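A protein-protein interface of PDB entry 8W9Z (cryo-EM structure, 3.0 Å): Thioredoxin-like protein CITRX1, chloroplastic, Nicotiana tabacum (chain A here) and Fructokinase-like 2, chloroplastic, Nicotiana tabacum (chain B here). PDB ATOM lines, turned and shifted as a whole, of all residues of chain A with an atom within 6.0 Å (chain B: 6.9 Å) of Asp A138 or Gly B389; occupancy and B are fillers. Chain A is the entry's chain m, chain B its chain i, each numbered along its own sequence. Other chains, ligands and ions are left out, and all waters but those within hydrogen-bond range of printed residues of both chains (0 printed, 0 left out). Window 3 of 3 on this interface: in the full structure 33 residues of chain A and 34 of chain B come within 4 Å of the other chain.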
ATOM      1  N   GLN A  81      12.529 -11.770  -5.265  1.00  0.00           N
ATOM      2  CA  GLN A  81      13.014 -10.693  -4.402  1.00  0.00           C
ATOM      3  C   GLN A  81      12.490 -10.853  -2.979  1.00  0.00           C
ATOM      4  O   GLN A  81      12.089  -9.898  -2.319  1.00  0.00           O
ATOM      5  CB  GLN A  81      12.618  -9.343  -4.989  1.00  0.00           C
ATOM      6  CG  GLN A  81      11.135  -9.220  -5.308  1.00  0.00           C
ATOM      7  CD  GLN A  81      10.785  -7.914  -5.996  1.00  0.00           C
ATOM      8  OE1 GLN A  81      11.635  -7.041  -6.169  1.00  0.00           O
ATOM      9  NE2 GLN A  81       9.525  -7.776  -6.394  1.00  0.00           N
ATOM     10  N   LYS A  85      15.546 -10.491   0.926  1.00  0.00           N
ATOM     11  CA  LYS A  85      14.963  -9.643   1.956  1.00  0.00           C
ATOM     12  C   LYS A  85      14.719 -10.392   3.259  1.00  0.00           C
ATOM     13  O   LYS A  85      14.450  -9.756   4.283  1.00  0.00           O
ATOM     14  CB  LYS A  85      13.649  -9.036   1.448  1.00  0.00           C
ATOM     15  CG  LYS A  85      13.180  -7.805   2.211  1.00  0.00           C
ATOM     16  CD  LYS A  85      14.180  -6.666   2.096  1.00  0.00           C
ATOM     17  CE  LYS A  85      14.334  -6.212   0.654  1.00  0.00           C
ATOM     18  NZ  LYS A  85      13.044  -5.742   0.077  1.00  0.00           N
ATOM     19  N   GLU A 134      12.205  -6.299 -16.704  1.00  0.00           N
ATOM     20  CA  GLU A 134      12.388  -5.196 -15.769  1.00  0.00           C
ATOM     21  C   GLU A 134      13.282  -5.581 -14.599  1.00  0.00           C
ATOM     22  O   GLU A 134      14.059  -4.752 -14.114  1.00  0.00           O
ATOM     23  CB  GLU A 134      11.031  -4.714 -15.249  1.00  0.00           C
ATOM     24  CG  GLU A 134      10.079  -4.243 -16.336  1.00  0.00           C
ATOM     25  CD  GLU A 134       8.735  -3.807 -15.785  1.00  0.00           C
ATOM     26  OE1 GLU A 134       8.546  -3.877 -14.553  1.00  0.00           O
ATOM     27  OE2 GLU A 134       7.869  -3.394 -16.585  1.00  0.00           O
ATOM     28  N   PHE A 135      13.190  -6.828 -14.139  1.00  0.00           N
ATOM     29  CA  PHE A 135      14.014  -7.307 -13.038  1.00  0.00           C
ATOM     30  C   PHE A 135      15.441  -7.624 -13.465  1.00  0.00           C
ATOM     31  O   PHE A 135      16.274  -7.935 -12.607  1.00  0.00           O
ATOM     32  CB  PHE A 135      13.371  -8.547 -12.410  1.00  0.00           C
ATOM     33  CG  PHE A 135      13.939  -8.916 -11.070  1.00  0.00           C
ATOM     34  CD1 PHE A 135      13.631  -8.171  -9.945  1.00  0.00           C
ATOM     35  CD2 PHE A 135      14.770 -10.016 -10.933  1.00  0.00           C
ATOM     36  CE1 PHE A 135      14.149  -8.509  -8.709  1.00  0.00           C
ATOM     37  CE2 PHE A 135      15.291 -10.359  -9.701  1.00  0.00           C
ATOM     38  CZ  PHE A 135      14.978  -9.605  -8.587  1.00  0.00           C
ATOM     39  N   ALA A 136      15.748  -7.541 -14.758  1.00  0.00           N
ATOM     40  CA  ALA A 136      17.089  -7.836 -15.243  1.00  0.00           C
ATOM     41  C   ALA A 136      17.961  -6.589 -15.337  1.00  0.00           C
ATOM     42  O   ALA A 136      19.147  -6.638 -14.993  1.00  0.00           O
ATOM     43  CB  ALA A 136      17.016  -8.523 -16.609  1.00  0.00           C
ATOM     44  N   ARG A 137      17.397  -5.468 -15.791  1.00  0.00           N
ATOM     45  CA  ARG A 137      18.200  -4.263 -15.975  1.00  0.00           C
ATOM     46  C   ARG A 137      18.655  -3.684 -14.640  1.00  0.00           C
ATOM     47  O   ARG A 137      19.776  -3.175 -14.530  1.00  0.00           O
ATOM     48  CB  ARG A 137      17.417  -3.227 -16.782  1.00  0.00           C
ATOM     49  CG  ARG A 137      16.027  -2.932 -16.248  1.00  0.00           C
ATOM     50  CD  ARG A 137      15.259  -2.036 -17.203  1.00  0.00           C
ATOM     51  NE  ARG A 137      15.147  -2.633 -18.531  1.00  0.00           N
ATOM     52  CZ  ARG A 137      14.538  -2.057 -19.562  1.00  0.00           C
ATOM     53  NH1 ARG A 137      13.982  -0.862 -19.421  1.00  0.00           N
ATOM     54  NH2 ARG A 137      14.485  -2.676 -20.733  1.00  0.00           N
ATOM     55  N   ASP A 138      17.803  -3.749 -13.613  1.00  0.00           N
ATOM     56  CA  ASP A 138      18.206  -3.280 -12.293  1.00  0.00           C
ATOM     57  C   ASP A 138      19.112  -4.272 -11.577  1.00  0.00           C
ATOM     58  O   ASP A 138      19.818  -3.884 -10.641  1.00  0.00           O
ATOM     59  CB  ASP A 138      16.976  -2.978 -11.434  1.00  0.00           C
ATOM     60  CG  ASP A 138      16.041  -4.164 -11.312  1.00  0.00           C
ATOM     61  OD1 ASP A 138      16.299  -5.194 -11.965  1.00  0.00           O
ATOM     62  OD2 ASP A 138      15.048  -4.065 -10.561  1.00  0.00           O
ATOM     63  N   MET A 139      19.106  -5.539 -11.995  1.00  0.00           N
ATOM     64  CA  MET A 139      20.057  -6.519 -11.486  1.00  0.00           C
ATOM     65  C   MET A 139      21.448  -6.330 -12.078  1.00  0.00           C
ATOM     66  O   MET A 139      22.381  -7.033 -11.671  1.00  0.00           O
ATOM     67  CB  MET A 139      19.540  -7.933 -11.774  1.00  0.00           C
ATOM     68  CG  MET A 139      20.224  -9.049 -10.995  1.00  0.00           C
ATOM     69  SD  MET A 139      20.153  -8.821  -9.209  1.00  0.00           S
ATOM     70  CE  MET A 139      18.386  -8.733  -8.945  1.00  0.00           C
ATOM     71  N   GLN A 140      21.605  -5.394 -13.016  1.00  0.00           N
ATOM     72  CA  GLN A 140      22.879  -5.113 -13.677  1.00  0.00           C
ATOM     73  C   GLN A 140      23.403  -6.353 -14.403  1.00  0.00           C
ATOM     74  O   GLN A 140      24.492  -6.862 -14.130  1.00  0.00           O
ATOM     75  CB  GLN A 140      23.911  -4.570 -12.682  1.00  0.00           C
ATOM     76  CG  GLN A 140      23.505  -3.263 -12.019  1.00  0.00           C
ATOM     77  CD  GLN A 140      23.384  -2.119 -13.007  1.00  0.00           C
ATOM     78  OE1 GLN A 140      24.008  -2.128 -14.068  1.00  0.00           O
ATOM     79  NE2 GLN A 140      22.575  -1.124 -12.661  1.00  0.00           N
ATOM     80  N   VAL A 141      22.596  -6.834 -15.342  1.00  0.00           N
ATOM     81  CA  VAL A 141      22.959  -7.964 -16.185  1.00  0.00           C
ATOM     82  C   VAL A 141      23.362  -7.435 -17.553  1.00  0.00           C
ATOM     83  O   VAL A 141      22.833  -6.429 -18.039  1.00  0.00           O
ATOM     84  CB  VAL A 141      21.807  -8.988 -16.288  1.00  0.00           C
ATOM     85  CG1 VAL A 141      20.680  -8.457 -17.159  1.00  0.00           C
ATOM     86  CG2 VAL A 141      22.320 -10.314 -16.814  1.00  0.00           C
ATOM     87  N   ILE B 385      24.150  -5.260  -2.607  1.00  0.00           N
ATOM     88  CA  ILE B 385      22.691  -5.288  -2.666  1.00  0.00           C
ATOM     89  C   ILE B 385      22.142  -3.895  -2.951  1.00  0.00           C
ATOM     90  O   ILE B 385      21.281  -3.715  -3.820  1.00  0.00           O
ATOM     91  CB  ILE B 385      22.109  -5.874  -1.366  1.00  0.00           C
ATOM     92  CG1 ILE B 385      22.192  -7.405  -1.371  1.00  0.00           C
ATOM     93  CG2 ILE B 385      20.668  -5.424  -1.171  1.00  0.00           C
ATOM     94  CD1 ILE B 385      23.559  -7.966  -1.032  1.00  0.00           C
ATOM     95  N   LYS B 387      20.158  -0.251  -2.313  1.00  0.00           N
ATOM     96  CA  LYS B 387      18.910   0.213  -1.722  1.00  0.00           C
ATOM     97  C   LYS B 387      17.772  -0.728  -2.113  1.00  0.00           C
ATOM     98  O   LYS B 387      17.986  -1.817  -2.650  1.00  0.00           O
ATOM     99  CB  LYS B 387      18.633   1.654  -2.144  1.00  0.00           C
ATOM    100  N   ARG B 388      16.538  -0.310  -1.839  1.00  0.00           N
ATOM    101  CA  ARG B 388      15.377  -1.122  -2.162  1.00  0.00           C
ATOM    102  C   ARG B 388      15.174  -1.200  -3.673  1.00  0.00           C
ATOM    103  O   ARG B 388      15.636  -0.349  -4.437  1.00  0.00           O
ATOM    104  CB  ARG B 388      14.124  -0.556  -1.494  1.00  0.00           C
ATOM    105  N   GLY B 389      14.469  -2.243  -4.098  1.00  0.00           N
ATOM    106  CA  GLY B 389      14.212  -2.472  -5.503  1.00  0.00           C
ATOM    107  C   GLY B 389      15.188  -3.395  -6.196  1.00  0.00           C
ATOM    108  O   GLY B 389      15.131  -3.512  -7.426  1.00  0.00           O
ATOM    109  N   GLY B 390      16.075  -4.052  -5.454  1.00  0.00           N
ATOM    110  CA  GLY B 390      17.040  -4.946  -6.062  1.00  0.00           C
ATOM    111  C   GLY B 390      18.045  -4.263  -6.962  1.00  0.00           C
ATOM    112  O   GLY B 390      18.597  -4.905  -7.862  1.00  0.00           O
ATOM    113  N   LEU B 391      18.319  -2.993  -6.703  1.00  0.00           N
ATOM    114  CA  LEU B 391      19.297  -2.267  -7.494  1.00  0.00           C
ATOM    115  C   LEU B 391      20.713  -2.638  -7.087  1.00  0.00           C
ATOM    116  O   LEU B 391      21.252  -2.086  -6.136  1.00  0.00           O
ATOM    117  CB  LEU B 391      19.076  -0.767  -7.353  1.00  0.00           C
ATOM    118  CG  LEU B 391      19.883   0.122  -8.300  1.00  0.00           C
ATOM    119  CD1 LEU B 391      19.665  -0.290  -9.747  1.00  0.00           C
ATOM    120  CD2 LEU B 391      19.518   1.582  -8.093  1.00  0.00           C
ATOM    121  N   ARG B 392      21.321  -3.570  -7.807  1.00  0.00           N
ATOM    122  CA  ARG B 392      22.681  -3.982  -7.500  1.00  0.00           C
ATOM    123  C   ARG B 392      23.716  -2.937  -7.842  1.00  0.00           C
ATOM    124  O   ARG B 392      23.509  -2.122  -8.733  1.00  0.00           O
ATOM    125  CB  ARG B 392      23.024  -5.276  -8.217  1.00  0.00           C
ATOM    126  CG  ARG B 392      22.299  -6.487  -7.674  1.00  0.00           C
ATOM    127  CD  ARG B 392      22.659  -6.707  -6.219  1.00  0.00           C
ATOM    128  NE  ARG B 392      21.764  -7.645  -5.552  1.00  0.00           N
ATOM    129  CZ  ARG B 392      20.618  -7.298  -4.975  1.00  0.00           C
ATOM    130  NH1 ARG B 392      20.219  -6.034  -4.990  1.00  0.00           N
ATOM    131  NH2 ARG B 392      19.866  -8.216  -4.384  1.00  0.00           N
ATOM    132  N   MET B 393      24.831  -2.947  -7.126  1.00  0.00           N
ATOM    133  CA  MET B 393      25.909  -2.018  -7.415  1.00  0.00           C
ATOM    134  C   MET B 393      27.131  -2.823  -7.757  1.00  0.00           C
ATOM    135  O   MET B 393      27.515  -3.687  -6.999  1.00  0.00           O
ATOM    136  CB  MET B 393      26.202  -1.171  -6.193  1.00  0.00           C
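O of Asp A138 is in hydrogen-bond range of N of Arg B392 (3.2 Å). The side-chain carboxylate of Asp A138 lies close to the backbone carbonyl oxygen of Gly B389. The backbone carbonyl oxygen (O) of Gly B390 sits close to the backbone carbonyl oxygen (O) of Asp A138.
Hydrophobic or aromatic side chains of chain A that line the printed part of chain B: Met A139. Hydrophobic or aromatic side chains of chain B that line the printed part of chain A: Leu B391. Among the printed residues, 7 pairs touch across the chains. Among the printed residues, no Asp or Glu carboxylate lies within 4 Å of a Lys or Arg side-chain nitrogen of the other chain.
Leu B391 touches Asp A138. Met A139 touches Gly B390. Met A139 touches Arg B392 (SD to CG, 3.5 Å). Arg B392 touches Gln A140 (O to CG, 3.5 Å).
Glu A134 touches none of the printed residues of chain B. Asp A138 touches just these residues of chain B: Gly B389 (3.2 Å), Gly B390 (3.2 Å), Leu B391 (3.6 Å) and Arg B392 (3.2 Å). Of the printed residues of chain B, Met A139 touches Gly B390 and Arg B392. Of the printed residues of chain B, Gln A140 touches Arg B392 (3.5 Å). Printed residues of chain A within 4 Å of Gly B390: Asp A138 (3.2 Å) and Met A139 (3.98 Å). Of the printed residues of chain A, Leu B391 touches Asp A138. Of the printed residues of chain A, Arg B392 touches Asp A138 (3.2 Å), Met A139 (3.5 Å) and Gln A140 (3.5 Å). The nearest residue of chain B that does not touch Asp A138 is Met B393 (6.2 Å).
The guanidinium group (NH1) of Arg B392 sits at hydrogen-bond distance from the backbone carbonyl oxygen (O) of Ile B385 (2.8 Å). The backbone carbonyl oxygen (O) of Gly B390 sits close to the guanidinium group (NH1) of Arg B392.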
